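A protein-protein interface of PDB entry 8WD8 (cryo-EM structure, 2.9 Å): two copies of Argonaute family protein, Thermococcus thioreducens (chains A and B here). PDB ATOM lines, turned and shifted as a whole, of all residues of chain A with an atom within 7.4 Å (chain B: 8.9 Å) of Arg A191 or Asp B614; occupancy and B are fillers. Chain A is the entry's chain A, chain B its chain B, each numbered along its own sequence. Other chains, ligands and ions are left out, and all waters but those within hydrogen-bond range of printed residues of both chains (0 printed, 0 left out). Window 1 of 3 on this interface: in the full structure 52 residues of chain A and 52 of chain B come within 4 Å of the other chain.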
ATOM      1  N   ILE A 188     -22.230 -38.809 -11.412  1.00  0.00           N
ATOM      2  CA  ILE A 188     -22.086 -37.402 -11.068  1.00  0.00           C
ATOM      3  C   ILE A 188     -20.668 -36.971 -11.419  1.00  0.00           C
ATOM      4  O   ILE A 188     -19.694 -37.616 -11.010  1.00  0.00           O
ATOM      5  CB  ILE A 188     -22.416 -37.154  -9.583  1.00  0.00           C
ATOM      6  CG1 ILE A 188     -23.925 -36.977  -9.420  1.00  0.00           C
ATOM      7  CG2 ILE A 188     -21.719 -35.913  -9.037  1.00  0.00           C
ATOM      8  CD1 ILE A 188     -24.428 -37.213  -8.025  1.00  0.00           C
ATOM      9  N   PHE A 189     -20.558 -35.905 -12.204  1.00  0.00           N
ATOM     10  CA  PHE A 189     -19.283 -35.347 -12.623  1.00  0.00           C
ATOM     11  C   PHE A 189     -19.039 -34.029 -11.901  1.00  0.00           C
ATOM     12  O   PHE A 189     -19.920 -33.501 -11.216  1.00  0.00           O
ATOM     13  CB  PHE A 189     -19.249 -35.124 -14.142  1.00  0.00           C
ATOM     14  CG  PHE A 189     -19.415 -36.384 -14.951  1.00  0.00           C
ATOM     15  CD1 PHE A 189     -20.677 -36.830 -15.320  1.00  0.00           C
ATOM     16  CD2 PHE A 189     -18.307 -37.118 -15.346  1.00  0.00           C
ATOM     17  CE1 PHE A 189     -20.831 -37.987 -16.062  1.00  0.00           C
ATOM     18  CE2 PHE A 189     -18.453 -38.278 -16.089  1.00  0.00           C
ATOM     19  CZ  PHE A 189     -19.718 -38.711 -16.447  1.00  0.00           C
ATOM     20  N   LYS A 190     -17.825 -33.506 -12.049  1.00  0.00           N
ATOM     21  CA  LYS A 190     -17.541 -32.162 -11.565  1.00  0.00           C
ATOM     22  C   LYS A 190     -18.261 -31.142 -12.437  1.00  0.00           C
ATOM     23  O   LYS A 190     -18.360 -31.311 -13.656  1.00  0.00           O
ATOM     24  CB  LYS A 190     -16.035 -31.900 -11.555  1.00  0.00           C
ATOM     25  CG  LYS A 190     -15.213 -33.046 -10.987  1.00  0.00           C
ATOM     26  CD  LYS A 190     -15.350 -33.128  -9.475  1.00  0.00           C
ATOM     27  CE  LYS A 190     -14.311 -34.056  -8.862  1.00  0.00           C
ATOM     28  NZ  LYS A 190     -13.159 -34.310  -9.772  1.00  0.00           N
ATOM     29  N   ARG A 191     -18.776 -30.088 -11.801  1.00  0.00           N
ATOM     30  CA  ARG A 191     -19.654 -29.154 -12.499  1.00  0.00           C
ATOM     31  C   ARG A 191     -18.874 -28.251 -13.446  1.00  0.00           C
ATOM     32  O   ARG A 191     -19.405 -27.809 -14.471  1.00  0.00           O
ATOM     33  CB  ARG A 191     -20.434 -28.320 -11.483  1.00  0.00           C
ATOM     34  CG  ARG A 191     -21.836 -27.945 -11.929  1.00  0.00           C
ATOM     35  CD  ARG A 191     -22.627 -27.347 -10.780  1.00  0.00           C
ATOM     36  NE  ARG A 191     -23.134 -28.375  -9.879  1.00  0.00           N
ATOM     37  CZ  ARG A 191     -24.045 -28.165  -8.939  1.00  0.00           C
ATOM     38  NH1 ARG A 191     -24.578 -26.969  -8.749  1.00  0.00           N
ATOM     39  NH2 ARG A 191     -24.431 -29.179  -8.172  1.00  0.00           N
ATOM     40  N   TYR A 192     -17.614 -27.967 -13.123  1.00  0.00           N
ATOM     41  CA  TYR A 192     -16.803 -27.045 -13.906  1.00  0.00           C
ATOM     42  C   TYR A 192     -15.526 -27.663 -14.449  1.00  0.00           C
ATOM     43  O   TYR A 192     -14.868 -27.047 -15.290  1.00  0.00           O
ATOM     44  CB  TYR A 192     -16.451 -25.813 -13.062  1.00  0.00           C
ATOM     45  CG  TYR A 192     -17.649 -25.245 -12.335  1.00  0.00           C
ATOM     46  CD1 TYR A 192     -18.777 -24.831 -13.036  1.00  0.00           C
ATOM     47  CD2 TYR A 192     -17.665 -25.148 -10.948  1.00  0.00           C
ATOM     48  CE1 TYR A 192     -19.881 -24.323 -12.380  1.00  0.00           C
ATOM     49  CE2 TYR A 192     -18.767 -24.640 -10.280  1.00  0.00           C
ATOM     50  CZ  TYR A 192     -19.870 -24.229 -11.003  1.00  0.00           C
ATOM     51  OH  TYR A 192     -20.970 -23.723 -10.352  1.00  0.00           O
ATOM     52  N   ASN A 193     -15.158 -28.860 -13.990  1.00  0.00           N
ATOM     53  CA  ASN A 193     -13.981 -29.535 -14.525  1.00  0.00           C
ATOM     54  C   ASN A 193     -14.372 -30.616 -15.528  1.00  0.00           C
ATOM     55  O   ASN A 193     -13.757 -30.736 -16.593  1.00  0.00           O
ATOM     56  CB  ASN A 193     -13.154 -30.132 -13.385  1.00  0.00           C
ATOM     57  CG  ASN A 193     -11.768 -30.557 -13.831  1.00  0.00           C
ATOM     58  OD1 ASN A 193     -11.289 -30.146 -14.888  1.00  0.00           O
ATOM     59  ND2 ASN A 193     -11.116 -31.385 -13.024  1.00  0.00           N
ATOM     60  N   GLY A 194     -15.391 -31.409 -15.203  1.00  0.00           N
ATOM     61  CA  GLY A 194     -15.859 -32.465 -16.076  1.00  0.00           C
ATOM     62  C   GLY A 194     -15.334 -33.848 -15.759  1.00  0.00           C
ATOM     63  O   GLY A 194     -15.687 -34.800 -16.464  1.00  0.00           O
ATOM     64  N   ASP A 195     -14.504 -33.989 -14.729  1.00  0.00           N
ATOM     65  CA  ASP A 195     -13.947 -35.284 -14.364  1.00  0.00           C
ATOM     66  C   ASP A 195     -14.994 -36.125 -13.635  1.00  0.00           C
ATOM     67  O   ASP A 195     -15.899 -35.576 -13.001  1.00  0.00           O
ATOM     68  CB  ASP A 195     -12.715 -35.101 -13.476  1.00  0.00           C
ATOM     69  CG  ASP A 195     -11.417 -35.261 -14.243  1.00  0.00           C
ATOM     70  OD1 ASP A 195     -11.322 -36.197 -15.063  1.00  0.00           O
ATOM     71  OD2 ASP A 195     -10.493 -34.450 -14.025  1.00  0.00           O
ATOM     72  N   ASP A 197     -16.459 -38.449 -10.612  1.00  0.00           N
ATOM     73  CA  ASP A 197     -16.286 -38.426  -9.163  1.00  0.00           C
ATOM     74  C   ASP A 197     -16.126 -39.858  -8.667  1.00  0.00           C
ATOM     75  O   ASP A 197     -17.115 -40.583  -8.511  1.00  0.00           O
ATOM     76  CB  ASP A 197     -17.470 -37.737  -8.490  1.00  0.00           C
ATOM     77  CG  ASP A 197     -17.038 -36.686  -7.488  1.00  0.00           C
ATOM     78  OD1 ASP A 197     -15.936 -36.823  -6.917  1.00  0.00           O
ATOM     79  OD2 ASP A 197     -17.803 -35.722  -7.269  1.00  0.00           O
ATOM     80  N   ARG A 251     -33.337 -37.353  -6.434  1.00  0.00           N
ATOM     81  CA  ARG A 251     -32.016 -37.019  -6.955  1.00  0.00           C
ATOM     82  C   ARG A 251     -31.095 -36.447  -5.885  1.00  0.00           C
ATOM     83  O   ARG A 251     -29.885 -36.347  -6.117  1.00  0.00           O
ATOM     84  CB  ARG A 251     -32.140 -36.027  -8.112  1.00  0.00           C
ATOM     85  CG  ARG A 251     -32.152 -36.667  -9.490  1.00  0.00           C
ATOM     86  CD  ARG A 251     -32.415 -35.643 -10.592  1.00  0.00           C
ATOM     87  NE  ARG A 251     -31.199 -34.962 -11.023  1.00  0.00           N
ATOM     88  CZ  ARG A 251     -30.788 -33.785 -10.568  1.00  0.00           C
ATOM     89  NH1 ARG A 251     -31.482 -33.108  -9.670  1.00  0.00           N
ATOM     90  NH2 ARG A 251     -29.652 -33.272 -11.033  1.00  0.00           N
ATOM     91  N   GLU B 576     -34.271 -24.709  -3.962  1.00  0.00           N
ATOM     92  CA  GLU B 576     -33.808 -23.408  -3.485  1.00  0.00           C
ATOM     93  C   GLU B 576     -32.282 -23.430  -3.552  1.00  0.00           C
ATOM     94  O   GLU B 576     -31.581 -23.708  -2.577  1.00  0.00           O
ATOM     95  CB  GLU B 576     -34.346 -23.123  -2.082  1.00  0.00           C
ATOM     96  CG  GLU B 576     -33.929 -21.780  -1.487  1.00  0.00           C
ATOM     97  CD  GLU B 576     -35.019 -21.147  -0.645  1.00  0.00           C
ATOM     98  OE1 GLU B 576     -36.118 -21.734  -0.553  1.00  0.00           O
ATOM     99  OE2 GLU B 576     -34.774 -20.066  -0.069  1.00  0.00           O
ATOM    100  N   SER B 577     -31.771 -23.159  -4.754  1.00  0.00           N
ATOM    101  CA  SER B 577     -30.333 -23.156  -5.015  1.00  0.00           C
ATOM    102  C   SER B 577     -30.098 -22.340  -6.278  1.00  0.00           C
ATOM    103  O   SER B 577     -30.506 -22.759  -7.365  1.00  0.00           O
ATOM    104  CB  SER B 577     -29.798 -24.576  -5.170  1.00  0.00           C
ATOM    105  OG  SER B 577     -29.458 -25.130  -3.911  1.00  0.00           O
ATOM    106  N   ILE B 578     -29.448 -21.193  -6.137  1.00  0.00           N
ATOM    107  CA  ILE B 578     -29.214 -20.302  -7.266  1.00  0.00           C
ATOM    108  C   ILE B 578     -27.990 -20.774  -8.039  1.00  0.00           C
ATOM    109  O   ILE B 578     -26.953 -21.101  -7.452  1.00  0.00           O
ATOM    110  CB  ILE B 578     -29.042 -18.851  -6.779  1.00  0.00           C
ATOM    111  CG1 ILE B 578     -30.161 -18.477  -5.800  1.00  0.00           C
ATOM    112  CG2 ILE B 578     -28.987 -17.885  -7.962  1.00  0.00           C
ATOM    113  CD1 ILE B 578     -31.465 -18.074  -6.454  1.00  0.00           C
ATOM    114  N   ASP B 579     -28.109 -20.830  -9.363  1.00  0.00           N
ATOM    115  CA  ASP B 579     -26.951 -21.062 -10.226  1.00  0.00           C
ATOM    116  C   ASP B 579     -26.240 -19.726 -10.397  1.00  0.00           C
ATOM    117  O   ASP B 579     -26.635 -18.884 -11.203  1.00  0.00           O
ATOM    118  CB  ASP B 579     -27.376 -21.656 -11.562  1.00  0.00           C
ATOM    119  CG  ASP B 579     -26.277 -22.474 -12.207  1.00  0.00           C
ATOM    120  OD1 ASP B 579     -26.080 -23.638 -11.800  1.00  0.00           O
ATOM    121  OD2 ASP B 579     -25.609 -21.953 -13.124  1.00  0.00           O
ATOM    122  N   MET B 580     -25.176 -19.525  -9.614  1.00  0.00           N
ATOM    123  CA  MET B 580     -24.484 -18.241  -9.605  1.00  0.00           C
ATOM    124  C   MET B 580     -23.643 -18.011 -10.852  1.00  0.00           C
ATOM    125  O   MET B 580     -23.320 -16.859 -11.154  1.00  0.00           O
ATOM    126  CB  MET B 580     -23.595 -18.120  -8.364  1.00  0.00           C
ATOM    127  CG  MET B 580     -24.283 -18.473  -7.057  1.00  0.00           C
ATOM    128  SD  MET B 580     -25.616 -17.327  -6.657  1.00  0.00           S
ATOM    129  CE  MET B 580     -24.970 -16.524  -5.198  1.00  0.00           C
ATOM    130  N   LYS B 581     -23.285 -19.077 -11.572  1.00  0.00           N
ATOM    131  CA  LYS B 581     -22.495 -18.936 -12.792  1.00  0.00           C
ATOM    132  C   LYS B 581     -23.300 -18.253 -13.893  1.00  0.00           C
ATOM    133  O   LYS B 581     -22.846 -17.269 -14.492  1.00  0.00           O
ATOM    134  CB  LYS B 581     -22.009 -20.313 -13.247  1.00  0.00           C
ATOM    135  CG  LYS B 581     -20.745 -20.307 -14.086  1.00  0.00           C
ATOM    136  CD  LYS B 581     -20.543 -21.652 -14.775  1.00  0.00           C
ATOM    137  CE  LYS B 581     -20.841 -21.583 -16.261  1.00  0.00           C
ATOM    138  NZ  LYS B 581     -20.725 -22.917 -16.915  1.00  0.00           N
ATOM    139  N   LYS B 610     -30.093 -18.885   3.473  1.00  0.00           N
ATOM    140  CA  LYS B 610     -28.757 -19.424   3.672  1.00  0.00           C
ATOM    141  C   LYS B 610     -28.116 -19.736   2.328  1.00  0.00           C
ATOM    142  O   LYS B 610     -28.773 -20.223   1.404  1.00  0.00           O
ATOM    143  CB  LYS B 610     -28.784 -20.683   4.548  1.00  0.00           C
ATOM    144  CG  LYS B 610     -28.708 -20.394   6.038  1.00  0.00           C
ATOM    145  CD  LYS B 610     -28.438 -21.654   6.839  1.00  0.00           C
ATOM    146  CE  LYS B 610     -29.370 -21.755   8.035  1.00  0.00           C
ATOM    147  NZ  LYS B 610     -29.254 -23.071   8.721  1.00  0.00           N
ATOM    148  N   ILE B 611     -26.822 -19.445   2.229  1.00  0.00           N
ATOM    149  CA  ILE B 611     -26.056 -19.736   1.023  1.00  0.00           C
ATOM    150  C   ILE B 611     -25.706 -21.219   1.009  1.00  0.00           C
ATOM    151  O   ILE B 611     -25.090 -21.733   1.950  1.00  0.00           O
ATOM    152  CB  ILE B 611     -24.790 -18.862   0.957  1.00  0.00           C
ATOM    153  CG1 ILE B 611     -25.166 -17.384   0.764  1.00  0.00           C
ATOM    154  CG2 ILE B 611     -23.811 -19.384  -0.104  1.00  0.00           C
ATOM    155  CD1 ILE B 611     -25.213 -16.904  -0.682  1.00  0.00           C
ATOM    156  N   THR B 612     -26.104 -21.911  -0.055  1.00  0.00           N
ATOM    157  CA  THR B 612     -25.833 -23.333  -0.175  1.00  0.00           C
ATOM    158  C   THR B 612     -24.404 -23.567  -0.669  1.00  0.00           C
ATOM    159  O   THR B 612     -23.662 -22.633  -0.980  1.00  0.00           O
ATOM    160  CB  THR B 612     -26.839 -23.995  -1.115  1.00  0.00           C
ATOM    161  OG1 THR B 612     -26.634 -23.520  -2.450  1.00  0.00           O
ATOM    162  CG2 THR B 612     -28.260 -23.672  -0.683  1.00  0.00           C
ATOM    163  N   LYS B 613     -24.022 -24.845  -0.736  1.00  0.00           N
ATOM    164  CA  LYS B 613     -22.667 -25.189  -1.153  1.00  0.00           C
ATOM    165  C   LYS B 613     -22.494 -25.052  -2.661  1.00  0.00           C
ATOM    166  O   LYS B 613     -21.400 -24.725  -3.139  1.00  0.00           O
ATOM    167  CB  LYS B 613     -22.323 -26.607  -0.698  1.00  0.00           C
ATOM    168  CG  LYS B 613     -22.712 -26.895   0.742  1.00  0.00           C
ATOM    169  CD  LYS B 613     -21.603 -26.496   1.701  1.00  0.00           C
ATOM    170  CE  LYS B 613     -22.129 -26.338   3.117  1.00  0.00           C
ATOM    171  NZ  LYS B 613     -22.651 -24.967   3.367  1.00  0.00           N
ATOM    172  N   ASP B 614     -23.563 -25.304  -3.424  1.00  0.00           N
ATOM    173  CA  ASP B 614     -23.509 -25.125  -4.873  1.00  0.00           C
ATOM    174  C   ASP B 614     -23.366 -23.654  -5.239  1.00  0.00           C
ATOM    175  O   ASP B 614     -22.651 -23.309  -6.189  1.00  0.00           O
ATOM    176  CB  ASP B 614     -24.758 -25.720  -5.521  1.00  0.00           C
ATOM    177  CG  ASP B 614     -25.058 -27.121  -5.027  1.00  0.00           C
ATOM    178  OD1 ASP B 614     -25.404 -27.269  -3.836  1.00  0.00           O
ATOM    179  OD2 ASP B 614     -24.949 -28.073  -5.828  1.00  0.00           O
ATOM    180  N   GLU B 615     -24.025 -22.772  -4.481  1.00  0.00           N
ATOM    181  CA  GLU B 615     -23.846 -21.335  -4.668  1.00  0.00           C
ATOM    182  C   GLU B 615     -22.427 -20.907  -4.318  1.00  0.00           C
ATOM    183  O   GLU B 615     -21.859 -20.028  -4.977  1.00  0.00           O
ATOM    184  CB  GLU B 615     -24.858 -20.560  -3.823  1.00  0.00           C
ATOM    185  CG  GLU B 615     -26.302 -20.755  -4.245  1.00  0.00           C
ATOM    186  CD  GLU B 615     -27.285 -20.107  -3.292  1.00  0.00           C
ATOM    187  OE1 GLU B 615     -26.846 -19.314  -2.433  1.00  0.00           O
ATOM    188  OE2 GLU B 615     -28.495 -20.390  -3.401  1.00  0.00           O
ATOM    189  N   GLU B 616     -21.836 -21.535  -3.297  1.00  0.00           N
ATOM    190  CA  GLU B 616     -20.456 -21.241  -2.916  1.00  0.00           C
ATOM    191  C   GLU B 616     -19.479 -21.659  -4.009  1.00  0.00           C
ATOM    192  O   GLU B 616     -18.542 -20.919  -4.336  1.00  0.00           O
ATOM    193  CB  GLU B 616     -20.127 -21.944  -1.599  1.00  0.00           C
ATOM    194  CG  GLU B 616     -19.467 -21.061  -0.558  1.00  0.00           C
ATOM    195  CD  GLU B 616     -19.027 -21.844   0.662  1.00  0.00           C
ATOM    196  OE1 GLU B 616     -19.608 -22.919   0.919  1.00  0.00           O
ATOM    197  OE2 GLU B 616     -18.102 -21.387   1.366  1.00  0.00           O
ATOM    198  N   GLU B 617     -19.699 -22.839  -4.602  1.00  0.00           N
ATOM    199  CA  GLU B 617     -18.843 -23.301  -5.693  1.00  0.00           C
ATOM    200  C   GLU B 617     -19.012 -22.441  -6.942  1.00  0.00           C
ATOM    201  O   GLU B 617     -18.032 -22.156  -7.643  1.00  0.00           O
ATOM    202  CB  GLU B 617     -19.140 -24.767  -6.008  1.00  0.00           C
ATOM    203  CG  GLU B 617     -18.743 -25.733  -4.905  1.00  0.00           C
ATOM    204  CD  GLU B 617     -19.410 -27.087  -5.051  1.00  0.00           C
ATOM    205  OE1 GLU B 617     -19.915 -27.386  -6.153  1.00  0.00           O
ATOM    206  OE2 GLU B 617     -19.429 -27.851  -4.063  1.00  0.00           O
ATOM    207  N   GLY B 618     -20.245 -22.002  -7.220  1.00  0.00           N
ATOM    208  CA  GLY B 618     -20.471 -21.117  -8.353  1.00  0.00           C
ATOM    209  C   GLY B 618     -19.834 -19.752  -8.176  1.00  0.00           C
ATOM    210  O   GLY B 618     -19.254 -19.203  -9.116  1.00  0.00           O
ATOM    211  N   LEU B 619     -19.911 -19.199  -6.960  1.00  0.00           N
ATOM    212  CA  LEU B 619     -19.267 -17.919  -6.681  1.00  0.00           C
ATOM    213  C   LEU B 619     -17.749 -18.040  -6.716  1.00  0.00           C
ATOM    214  O   LEU B 619     -17.060 -17.111  -7.154  1.00  0.00           O
ATOM    215  CB  LEU B 619     -19.724 -17.382  -5.326  1.00  0.00           C
ATOM    216  CG  LEU B 619     -21.136 -16.807  -5.222  1.00  0.00           C
ATOM    217  CD1 LEU B 619     -21.501 -16.592  -3.763  1.00  0.00           C
ATOM    218  CD2 LEU B 619     -21.252 -15.517  -6.010  1.00  0.00           C
ATOM    219  N   ALA B 620     -17.212 -19.186  -6.280  1.00  0.00           N
ATOM    220  CA  ALA B 620     -15.771 -19.413  -6.360  1.00  0.00           C
ATOM    221  C   ALA B 620     -15.302 -19.518  -7.808  1.00  0.00           C
ATOM    222  O   ALA B 620     -14.255 -18.965  -8.168  1.00  0.00           O
ATOM    223  CB  ALA B 620     -15.394 -20.671  -5.580  1.00  0.00           C
ATOM    224  N   TYR B 621     -16.079 -20.203  -8.656  1.00  0.00           N
ATOM    225  CA  TYR B 621     -15.727 -20.305 -10.073  1.00  0.00           C
ATOM    226  C   TYR B 621     -15.832 -18.954 -10.774  1.00  0.00           C
ATOM    227  O   TYR B 621     -14.992 -18.622 -11.620  1.00  0.00           O
ATOM    228  CB  TYR B 621     -16.618 -21.339 -10.763  1.00  0.00           C
ATOM    229  CG  TYR B 621     -16.342 -21.504 -12.243  1.00  0.00           C
ATOM    230  CD1 TYR B 621     -15.237 -22.223 -12.686  1.00  0.00           C
ATOM    231  CD2 TYR B 621     -17.191 -20.952 -13.198  1.00  0.00           C
ATOM    232  CE1 TYR B 621     -14.978 -22.381 -14.037  1.00  0.00           C
ATOM    233  CE2 TYR B 621     -16.939 -21.101 -14.551  1.00  0.00           C
ATOM    234  CZ  TYR B 621     -15.834 -21.817 -14.964  1.00  0.00           C
ATOM    235  OH  TYR B 621     -15.582 -21.970 -16.307  1.00  0.00           O
ATOM    236  N   ILE B 622     -16.851 -18.159 -10.423  1.00  0.00           N
ATOM    237  CA  ILE B 622     -17.013 -16.826 -11.003  1.00  0.00           C
ATOM    238  C   ILE B 622     -15.874 -15.907 -10.568  1.00  0.00           C
ATOM    239  O   ILE B 622     -15.317 -15.158 -11.383  1.00  0.00           O
ATOM    240  CB  ILE B 622     -18.400 -16.259 -10.629  1.00  0.00           C
ATOM    241  CG1 ILE B 622     -19.488 -16.915 -11.485  1.00  0.00           C
ATOM    242  CG2 ILE B 622     -18.465 -14.742 -10.772  1.00  0.00           C
ATOM    243  CD1 ILE B 622     -19.336 -16.662 -12.969  1.00  0.00           C
ATOM    244  N   ILE B 687     -12.438 -19.238  -0.661  1.00  0.00           N
ATOM    245  CA  ILE B 687     -13.471 -18.725   0.233  1.00  0.00           C
ATOM    246  C   ILE B 687     -12.931 -18.719   1.656  1.00  0.00           C
ATOM    247  O   ILE B 687     -12.561 -19.770   2.193  1.00  0.00           O
ATOM    248  CB  ILE B 687     -14.756 -19.563   0.140  1.00  0.00           C
ATOM    249  CG1 ILE B 687     -15.160 -19.767  -1.321  1.00  0.00           C
ATOM    250  CG2 ILE B 687     -15.878 -18.899   0.918  1.00  0.00           C
ATOM    251  CD1 ILE B 687     -15.497 -21.200  -1.665  1.00  0.00           C
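NH2 of Arg A191 lies within salt-bridge range of OD2 of Asp B614.
CE1 of Tyr A192 touches CD of Lys B581, 3.6 Å away. Glu B617 touches Tyr A192. CA of Gly B618 touches OH of Tyr A192, at 3.3 Å. Tyr A192 touches Tyr B621 (CB to CD1, 3.8 Å).
Phe A189 touches none of the printed residues of chain B. Arg A191 touches one residue of chain B. Of the printed residues of chain B, Tyr A192 touches Lys B581 (3.6 Å), Glu B617 (3.7 Å), Gly B618 (3.3 Å) and Tyr B621 (3.8 Å). Printed residues of chain A within 4 Å of Lys B581: Tyr A192 (3.6 Å). Of chain A, only Arg A191 (2.6 Å) comes within 4 Å of Asp B614. Glu B616 touches none of the printed residues of chain A. Of the printed residues of chain A, Glu B617 touches Tyr A192 (3.7 Å). Of the printed residues of chain A, Gly B618 touches Tyr A192. Printed residues of chain A within 4 Å of Tyr B621: Tyr A192 (3.8 Å). The nearest printed residue of chain A that does not touch Glu B617 is Arg A191 (5.0 Å).
Of the 10 printed residues of chain A, 2 touch a printed residue of chain B. Hydrophobic or aromatic side chains of chain A within 4 Å of the printed part of chain B: Tyr A192. Hydrophobic or aromatic side chains of chain B within 4 Å of the printed part of chain A: Tyr B621. Among the printed residues, 5 pairs touch across the chains.
No position is printed for both chains.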
